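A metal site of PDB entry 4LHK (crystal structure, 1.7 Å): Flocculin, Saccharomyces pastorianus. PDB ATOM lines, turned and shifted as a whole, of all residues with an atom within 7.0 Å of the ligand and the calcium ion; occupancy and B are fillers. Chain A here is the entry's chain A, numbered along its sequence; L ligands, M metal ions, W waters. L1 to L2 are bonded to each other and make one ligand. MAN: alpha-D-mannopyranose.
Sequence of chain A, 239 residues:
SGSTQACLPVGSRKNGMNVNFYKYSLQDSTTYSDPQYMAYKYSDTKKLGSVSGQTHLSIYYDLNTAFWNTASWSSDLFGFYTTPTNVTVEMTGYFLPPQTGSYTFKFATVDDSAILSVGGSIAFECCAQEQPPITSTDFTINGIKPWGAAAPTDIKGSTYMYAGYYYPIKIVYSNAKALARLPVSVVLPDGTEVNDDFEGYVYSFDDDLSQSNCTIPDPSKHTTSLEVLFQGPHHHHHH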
ATOM      1  N   SER A  29      -5.074  19.957   1.884  1.00  0.00           N
ATOM      2  CA  SER A  29      -4.645  19.343   3.126  1.00  0.00           C
ATOM      3  C   SER A  29      -3.967  17.988   2.929  1.00  0.00           C
ATOM      4  O   SER A  29      -3.674  17.241   3.892  1.00  0.00           O
ATOM      5  CB  SER A  29      -5.828  19.257   4.075  1.00  0.00           C
ATOM      6  OG  SER A  29      -6.826  18.488   3.454  1.00  0.00           O
ATOM      7  N   TYR A  32       0.888  18.747   0.808  1.00  0.00           N
ATOM      8  CA  TYR A  32       2.039  19.219   1.633  1.00  0.00           C
ATOM      9  C   TYR A  32       2.706  18.073   2.454  1.00  0.00           C
ATOM     10  O   TYR A  32       3.856  18.188   2.853  1.00  0.00           O
ATOM     11  CB  TYR A  32       1.566  20.346   2.564  1.00  0.00           C
ATOM     12  CG  TYR A  32       0.883  19.883   3.794  1.00  0.00           C
ATOM     13  CD1 TYR A  32      -0.410  19.377   3.757  1.00  0.00           C
ATOM     14  CD2 TYR A  32       1.520  19.934   5.050  1.00  0.00           C
ATOM     15  CE1 TYR A  32      -1.037  18.957   4.905  1.00  0.00           C
ATOM     16  CE2 TYR A  32       0.877  19.490   6.196  1.00  0.00           C
ATOM     17  CZ  TYR A  32      -0.366  19.003   6.122  1.00  0.00           C
ATOM     18  OH  TYR A  32      -1.005  18.574   7.253  1.00  0.00           O
ATOM     19  N   TRP A  68      -7.796  33.949   7.362  1.00  0.00           N
ATOM     20  CA  TRP A  68      -7.109  32.669   7.281  1.00  0.00           C
ATOM     21  C   TRP A  68      -7.634  31.642   6.283  1.00  0.00           C
ATOM     22  O   TRP A  68      -6.859  30.753   5.917  1.00  0.00           O
ATOM     23  CB  TRP A  68      -7.063  32.028   8.696  1.00  0.00           C
ATOM     24  CG  TRP A  68      -6.067  32.615   9.547  1.00  0.00           C
ATOM     25  CD1 TRP A  68      -5.340  33.783   9.355  1.00  0.00           C
ATOM     26  CD2 TRP A  68      -5.620  32.058  10.790  1.00  0.00           C
ATOM     27  NE1 TRP A  68      -4.473  33.975  10.438  1.00  0.00           N
ATOM     28  CE2 TRP A  68      -4.637  32.937  11.316  1.00  0.00           C
ATOM     29  CE3 TRP A  68      -5.977  30.920  11.516  1.00  0.00           C
ATOM     30  CZ2 TRP A  68      -3.957  32.656  12.588  1.00  0.00           C
ATOM     31  CZ3 TRP A  68      -5.329  30.662  12.768  1.00  0.00           C
ATOM     32  CH2 TRP A  68      -4.319  31.515  13.259  1.00  0.00           C
ATOM     33  N   ASN A  69      -8.879  31.751   5.828  1.00  0.00           N
ATOM     34  CA  ASN A  69      -9.408  30.832   4.781  1.00  0.00           C
ATOM     35  C   ASN A  69      -9.198  31.398   3.392  1.00  0.00           C
ATOM     36  O   ASN A  69      -9.802  30.931   2.450  1.00  0.00           O
ATOM     37  CB  ASN A  69     -10.873  30.508   5.064  1.00  0.00           C
ATOM     38  CG  ASN A  69     -11.037  29.852   6.420  1.00  0.00           C
ATOM     39  OD1 ASN A  69     -10.180  29.083   6.866  1.00  0.00           O
ATOM     40  ND2 ASN A  69     -12.132  30.148   7.088  1.00  0.00           N
ATOM     41  N   PRO A  84       1.756  34.258   0.040  1.00  0.00           N
ATOM     42  CA  PRO A  84       2.504  33.389   0.928  1.00  0.00           C
ATOM     43  C   PRO A  84       1.634  32.521   1.818  1.00  0.00           C
ATOM     44  O   PRO A  84       2.135  31.684   2.538  1.00  0.00           O
ATOM     45  CB  PRO A  84       3.331  34.369   1.767  1.00  0.00           C
ATOM     46  CG  PRO A  84       2.722  35.685   1.604  1.00  0.00           C
ATOM     47  CD  PRO A  84       2.123  35.665   0.220  1.00  0.00           C
ATOM     48  N   THR A  85       0.339  32.782   1.777  1.00  0.00           N
ATOM     49  CA  THR A  85      -0.692  31.927   2.373  1.00  0.00           C
ATOM     50  C   THR A  85      -0.679  30.527   1.757  1.00  0.00           C
ATOM     51  O   THR A  85      -1.104  29.526   2.404  1.00  0.00           O
ATOM     52  CB  THR A  85      -2.091  32.536   2.139  1.00  0.00           C
ATOM     53  OG1 THR A  85      -2.151  32.978   0.772  1.00  0.00           O
ATOM     54  CG2 THR A  85      -2.344  33.741   3.123  1.00  0.00           C
ATOM     55  N   ASP A 111       5.073  25.108   9.974  1.00  0.00           N
ATOM     56  CA  ASP A 111       3.704  25.317   9.583  1.00  0.00           C
ATOM     57  C   ASP A 111       3.776  25.749   8.131  1.00  0.00           C
ATOM     58  O   ASP A 111       4.173  26.914   7.895  1.00  0.00           O
ATOM     59  CB  ASP A 111       3.006  26.378  10.466  1.00  0.00           C
ATOM     60  CG  ASP A 111       1.543  26.635  10.069  1.00  0.00           C
ATOM     61  OD1 ASP A 111       1.210  26.283   8.917  1.00  0.00           O
ATOM     62  OD2 ASP A 111       0.762  27.197  10.902  1.00  0.00           O
ATOM     63  N   ASP A 112       3.517  24.872   7.148  1.00  0.00           N
ATOM     64  CA  ASP A 112       2.829  23.543   7.294  1.00  0.00           C
ATOM     65  C   ASP A 112       3.731  22.305   7.162  1.00  0.00           C
ATOM     66  O   ASP A 112       3.495  21.317   7.866  1.00  0.00           O
ATOM     67  CB  ASP A 112       1.674  23.452   6.292  1.00  0.00           C
ATOM     68  CG  ASP A 112       0.529  24.268   6.706  1.00  0.00           C
ATOM     69  OD1 ASP A 112      -0.283  23.793   7.534  1.00  0.00           O
ATOM     70  OD2 ASP A 112       0.388  25.374   6.131  1.00  0.00           O
ATOM     71  N   LYS A 145       3.243  19.592   9.999  1.00  0.00           N
ATOM     72  CA  LYS A 145       2.197  20.014  10.916  1.00  0.00           C
ATOM     73  C   LYS A 145       0.909  19.243  10.586  1.00  0.00           C
ATOM     74  O   LYS A 145       0.424  19.298   9.426  1.00  0.00           O
ATOM     75  CB  LYS A 145       1.943  21.512  10.803  1.00  0.00           C
ATOM     76  CG  LYS A 145       0.866  22.015  11.754  1.00  0.00           C
ATOM     77  CD  LYS A 145       0.590  23.475  11.488  1.00  0.00           C
ATOM     78  CE  LYS A 145      -0.380  24.056  12.504  1.00  0.00           C
ATOM     79  NZ  LYS A 145      -1.662  23.343  12.665  1.00  0.00           N
ATOM     80  N   PRO A 146       0.372  18.510  11.568  1.00  0.00           N
ATOM     81  CA  PRO A 146      -0.909  17.817  11.312  1.00  0.00           C
ATOM     82  C   PRO A 146      -1.955  18.856  11.021  1.00  0.00           C
ATOM     83  O   PRO A 146      -1.948  19.959  11.609  1.00  0.00           O
ATOM     84  CB  PRO A 146      -1.211  17.163  12.638  1.00  0.00           C
ATOM     85  CG  PRO A 146       0.108  17.043  13.328  1.00  0.00           C
ATOM     86  CD  PRO A 146       0.905  18.240  12.928  1.00  0.00           C
ATOM     87  N   TRP A 147      -2.899  18.507  10.182  1.00  0.00           N
ATOM     88  CA  TRP A 147      -3.906  19.448   9.766  1.00  0.00           C
ATOM     89  C   TRP A 147      -4.791  19.876  10.944  1.00  0.00           C
ATOM     90  O   TRP A 147      -5.527  19.058  11.520  1.00  0.00           O
ATOM     91  CB  TRP A 147      -4.743  18.886   8.591  1.00  0.00           C
ATOM     92  CG  TRP A 147      -5.505  19.952   7.943  1.00  0.00           C
ATOM     93  CD1 TRP A 147      -6.801  20.288   8.164  1.00  0.00           C
ATOM     94  CD2 TRP A 147      -4.987  20.876   7.021  1.00  0.00           C
ATOM     95  NE1 TRP A 147      -7.147  21.364   7.397  1.00  0.00           N
ATOM     96  CE2 TRP A 147      -6.034  21.747   6.673  1.00  0.00           C
ATOM     97  CE3 TRP A 147      -3.733  21.027   6.400  1.00  0.00           C
ATOM     98  CZ2 TRP A 147      -5.872  22.797   5.750  1.00  0.00           C
ATOM     99  CZ3 TRP A 147      -3.557  22.119   5.495  1.00  0.00           C
ATOM    100  CH2 TRP A 147      -4.635  22.957   5.177  1.00  0.00           C
ATOM    101  N   GLY A 148      -4.727  21.158  11.291  1.00  0.00           N
ATOM    102  CA  GLY A 148      -5.489  21.721  12.366  1.00  0.00           C
ATOM    103  C   GLY A 148      -5.053  21.429  13.785  1.00  0.00           C
ATOM    104  O   GLY A 148      -5.805  21.699  14.722  1.00  0.00           O
ATOM    105  N   ALA A 149      -3.874  20.854  13.970  1.00  0.00           N
ATOM    106  CA  ALA A 149      -3.358  20.555  15.291  1.00  0.00           C
ATOM    107  C   ALA A 149      -1.894  20.948  15.401  1.00  0.00           C
ATOM    108  O   ALA A 149      -1.190  21.264  14.427  1.00  0.00           O
ATOM    109  CB  ALA A 149      -3.512  19.080  15.618  1.00  0.00           C
ATOM    110  N   ALA A 150      -1.439  20.919  16.644  1.00  0.00           N
ATOM    111  CA  ALA A 150      -0.098  21.351  16.975  1.00  0.00           C
ATOM    112  C   ALA A 150       0.985  20.649  16.163  1.00  0.00           C
ATOM    113  O   ALA A 150       0.973  19.436  15.963  1.00  0.00           O
ATOM    114  CB  ALA A 150       0.166  21.193  18.463  1.00  0.00           C
ATOM    115  N   ALA A 151       1.930  21.454  15.709  1.00  0.00           N
ATOM    116  CA  ALA A 151       3.107  20.972  15.034  1.00  0.00           C
ATOM    117  C   ALA A 151       4.130  20.439  16.056  1.00  0.00           C
ATOM    118  O   ALA A 151       4.225  20.983  17.171  1.00  0.00           O
ATOM    119  CB  ALA A 151       3.699  22.115  14.223  1.00  0.00           C
ATOM    120  N   TYR A 173       9.898  23.950   1.677  1.00  0.00           N
ATOM    121  CA  TYR A 173       8.935  24.407   2.661  1.00  0.00           C
ATOM    122  C   TYR A 173       7.571  24.658   2.000  1.00  0.00           C
ATOM    123  O   TYR A 173       7.549  25.234   0.897  1.00  0.00           O
ATOM    124  CB  TYR A 173       9.444  25.726   3.358  1.00  0.00           C
ATOM    125  CG  TYR A 173       8.283  26.348   4.074  1.00  0.00           C
ATOM    126  CD1 TYR A 173       7.891  25.899   5.303  1.00  0.00           C
ATOM    127  CD2 TYR A 173       7.538  27.374   3.481  1.00  0.00           C
ATOM    128  CE1 TYR A 173       6.766  26.391   5.920  1.00  0.00           C
ATOM    129  CE2 TYR A 173       6.403  27.866   4.051  1.00  0.00           C
ATOM    130  CZ  TYR A 173       6.026  27.389   5.290  1.00  0.00           C
ATOM    131  OH  TYR A 173       4.896  27.914   5.812  1.00  0.00           O
ATOM    132  N   SER A 174       6.471  24.254   2.628  1.00  0.00           N
ATOM    133  CA  SER A 174       5.132  24.544   2.096  1.00  0.00           C
ATOM    134  C   SER A 174       4.213  25.158   3.108  1.00  0.00           C
ATOM    135  O   SER A 174       4.137  24.700   4.261  1.00  0.00           O
ATOM    136  CB  SER A 174       4.466  23.258   1.560  1.00  0.00           C
ATOM    137  OG  SER A 174       5.199  22.826   0.486  1.00  0.00           O
ATOM    138  N   ASN A 175       3.446  26.167   2.648  1.00  0.00           N
ATOM    139  CA  ASN A 175       2.338  26.735   3.384  1.00  0.00           C
ATOM    140  C   ASN A 175       1.089  26.431   2.626  1.00  0.00           C
ATOM    141  O   ASN A 175       1.042  26.658   1.436  1.00  0.00           O
ATOM    142  CB  ASN A 175       2.457  28.244   3.595  1.00  0.00           C
ATOM    143  CG  ASN A 175       1.462  28.763   4.647  1.00  0.00           C
ATOM    144  OD1 ASN A 175       0.903  28.013   5.378  1.00  0.00           O
ATOM    145  ND2 ASN A 175       1.251  30.043   4.679  1.00  0.00           N
ATOM    146  N   ALA A 176       0.127  25.826   3.304  1.00  0.00           N
ATOM    147  CA  ALA A 176      -1.124  25.394   2.702  1.00  0.00           C
ATOM    148  C   ALA A 176      -2.238  26.388   2.922  1.00  0.00           C
ATOM    149  O   ALA A 176      -3.188  26.453   2.147  1.00  0.00           O
ATOM    150  CB  ALA A 176      -1.476  24.045   3.276  1.00  0.00           C
ATOM    151  N   LYS A 177      -2.104  27.174   3.986  1.00  0.00           N
ATOM    152  CA  LYS A 177      -3.007  28.240   4.319  1.00  0.00           C
ATOM    153  C   LYS A 177      -2.517  29.075   5.502  1.00  0.00           C
ATOM    154  O   LYS A 177      -1.758  28.570   6.345  1.00  0.00           O
ATOM    155  CB  LYS A 177      -4.452  27.787   4.656  1.00  0.00           C
ATOM    156  CG  LYS A 177      -4.601  26.979   5.895  1.00  0.00           C
ATOM    157  CD  LYS A 177      -6.026  26.468   6.078  1.00  0.00           C
ATOM    158  CE  LYS A 177      -7.025  27.575   6.392  1.00  0.00           C
ATOM    159  NZ  LYS A 177      -8.376  27.023   6.720  1.00  0.00           N
ATOM    160  N   ALA A 178      -2.951  30.329   5.548  1.00  0.00           N
ATOM    161  CA  ALA A 178      -2.784  31.174   6.713  1.00  0.00           C
ATOM    162  C   ALA A 178      -1.247  31.384   7.065  1.00  0.00           C
ATOM    163  O   ALA A 178      -0.440  31.754   6.176  1.00  0.00           O
ATOM    164  CB  ALA A 178      -3.636  30.651   7.853  1.00  0.00           C
ATOM    165  N   LEU A 179      -0.863  31.078   8.287  1.00  0.00           N
ATOM    166  CA  LEU A 179       0.463  31.417   8.826  1.00  0.00           C
ATOM    167  C   LEU A 179       1.499  30.532   8.175  1.00  0.00           C
ATOM    168  O   LEU A 179       1.264  29.357   7.910  1.00  0.00           O
ATOM    169  CB  LEU A 179       0.504  31.103  10.331  1.00  0.00           C
ATOM    170  CG  LEU A 179      -0.518  31.602  11.270  1.00  0.00           C
ATOM    171  CD1 LEU A 179      -0.092  31.341  12.732  1.00  0.00           C
ATOM    172  CD2 LEU A 179      -0.710  33.067  10.956  1.00  0.00           C
ATOM    173  N   ALA A 180       2.641  31.123   7.906  1.00  0.00           N
ATOM    174  CA  ALA A 180       3.865  30.378   7.567  1.00  0.00           C
ATOM    175  C   ALA A 180       4.928  30.501   8.697  1.00  0.00           C
ATOM    176  O   ALA A 180       5.260  31.602   9.148  1.00  0.00           O
ATOM    177  CB  ALA A 180       4.407  30.891   6.245  1.00  0.00           C
ATOM    178  N   ARG A 181       5.473  29.373   9.108  1.00  0.00           N
ATOM    179  CA  ARG A 181       6.472  29.355  10.152  1.00  0.00           C
ATOM    180  C   ARG A 181       7.548  28.298   9.844  1.00  0.00           C
ATOM    181  O   ARG A 181       7.219  27.106   9.650  1.00  0.00           O
ATOM    182  CB  ARG A 181       5.922  28.948  11.538  1.00  0.00           C
ATOM    183  CG  ARG A 181       5.024  29.842  12.318  1.00  0.00           C
ATOM    184  CD  ARG A 181       4.928  29.306  13.785  1.00  0.00           C
ATOM    185  NE  ARG A 181       6.103  29.596  14.665  1.00  0.00           N
ATOM    186  CZ  ARG A 181       6.080  29.497  15.997  1.00  0.00           C
ATOM    187  NH1 ARG A 181       5.001  29.095  16.651  1.00  0.00           N
ATOM    188  NH2 ARG A 181       7.193  29.803  16.725  1.00  0.00           N
HETATM  189  C1  MAN L   1      -4.635  26.765  10.751  1.00  0.00           C
HETATM  190  C2  MAN L   1      -3.345  27.628  10.750  1.00  0.00           C
HETATM  191  C3  MAN L   1      -2.565  27.363   9.482  1.00  0.00           C
HETATM  192  C4  MAN L   1      -2.364  25.867   9.240  1.00  0.00           C
HETATM  193  C5  MAN L   1      -3.679  25.096   9.301  1.00  0.00           C
HETATM  194  C6  MAN L   1      -3.630  23.569   9.032  1.00  0.00           C
HETATM  195  O1  MAN L   1      -5.520  27.371   9.804  1.00  0.00           O
HETATM  196  O2  MAN L   1      -2.511  27.354  11.803  1.00  0.00           O
HETATM  197  O3  MAN L   1      -1.329  28.057   9.478  1.00  0.00           O
HETATM  198  O4  MAN L   1      -1.781  25.737   8.000  1.00  0.00           O
HETATM  199  O5  MAN L   1      -4.323  25.371  10.553  1.00  0.00           O
HETATM  200  O6  MAN L   1      -2.841  22.941  10.037  1.00  0.00           O
HETATM  201  C1  MAN L   2      -3.075  28.026  12.953  1.00  0.00           C
HETATM  202  C2  MAN L   2      -2.062  28.055  14.051  1.00  0.00           C
HETATM  203  C3  MAN L   2      -1.746  26.590  14.398  1.00  0.00           C
HETATM  204  C4  MAN L   2      -3.005  25.758  14.753  1.00  0.00           C
HETATM  205  C5  MAN L   2      -4.097  26.004  13.691  1.00  0.00           C
HETATM  206  C6  MAN L   2      -5.489  25.412  14.007  1.00  0.00           C
HETATM  207  O2  MAN L   2      -2.747  28.696  15.095  1.00  0.00           O
HETATM  208  O3  MAN L   2      -0.863  26.633  15.491  1.00  0.00           O
HETATM  209  O4  MAN L   2      -2.791  24.350  14.827  1.00  0.00           O
HETATM  210  O5  MAN L   2      -4.233  27.408  13.479  1.00  0.00           O
HETATM  211  O6  MAN L   2      -5.901  25.861  15.279  1.00  0.00           O
HETATM  212 CA    CA M   1      -0.052  27.479   7.350  1.00  0.00          CA
HETATM  213  O   HOH W   1      -4.992  28.851  16.297  1.00  0.00           O
HETATM  214  O   HOH W   2      -1.152  21.526   8.684  1.00  0.00           O
HETATM  215  O   HOH W   3       1.405  27.013  13.554  1.00  0.00           O
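O of Ala 149 sits at hydrogen-bond distance from O4 of MAN L2, 3.5 Å away. The backbone NH (N) of Leu 179 lies close to an oxygen (O3) of MAN L1, at 3.3 Å. The side-chain amino group (NZ) of Lys 145 is in hydrogen-bond range of an oxygen (O4) of MAN L2, at 2.6 Å. The backbone carbonyl oxygen (O) of Pro 146 sits at hydrogen-bond distance from an oxygen (O6) of MAN L1, 3.5 Å away. The backbone NH (N) of Gly 148 lies within hydrogen-bond range of an oxygen (O6) of MAN L1 (2.9 Å).
The backbone NH of Ala 176 sits close to the side-chain carboxylate of Asp 112, at 2.9 Å. The backbone carbonyl oxygen (O) of Pro 84 is in hydrogen-bond range of the side-chain amide nitrogen (ND2) of Asn 175 (2.8 Å). OH of Tyr 32 lies within hydrogen-bond range of N of Trp 147 (3.5 Å). OH of Tyr 173 lies within hydrogen-bond range of O of Asp 111. The backbone NH of Asp 112 lies within hydrogen-bond range of the backbone carbonyl oxygen of Ser 174 (3.0 Å). The side-chain amide nitrogen of Asn 175 lies within hydrogen-bond range of the backbone carbonyl oxygen of Ala 178 (2.8 Å). The backbone NH (N) of Lys 177 sits close to the backbone carbonyl oxygen (O) of Thr 85 (3.0 Å). The backbone carbonyl oxygen (O) of Ala 149 lies within hydrogen-bond range of the side-chain amino group (NZ) of Lys 145 (2.8 Å).
CZ3 of Trp 68 touches C1 of MAN L2, 3.5 Å away. CD2 of Trp 147 touches C6 of MAN L1, 3.6 Å away. CB of Ala 178 touches C3 of MAN L1 (3.8 Å). 11 residues have an atom within 4 Å of the ligand: Trp 68, Asp 111, Asp 112, Lys 145, Pro 146, Trp 147, Gly 148, Ala 149, Lys 177, Ala 178 and Leu 179.
Within 4 Å of the calcium ion: Asp 111, Asp 112, Asn 175, Lys 177 and Leu 179.
The calcium ion is bound by OD1 of Asn 175 (2.3 Å). O of Lys 177 binds the calcium ion, 2.3 Å away. The calcium ion is bound by OD1 of Asp 111, at 2.3 Å. O of Leu 179 binds the calcium ion (2.4 Å). OD2 of Asp 112 is bound to the calcium ion (2.5 Å). The calcium ion is bound by an oxygen (O4) of MAN L1 (2.5 Å). O3 of MAN L1 binds the calcium ion (2.5 Å).
Water W3 lies within hydrogen-bond range of OD2 of Asp 111 (2.7 Å) and O3 of MAN L2 (3.0 Å).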
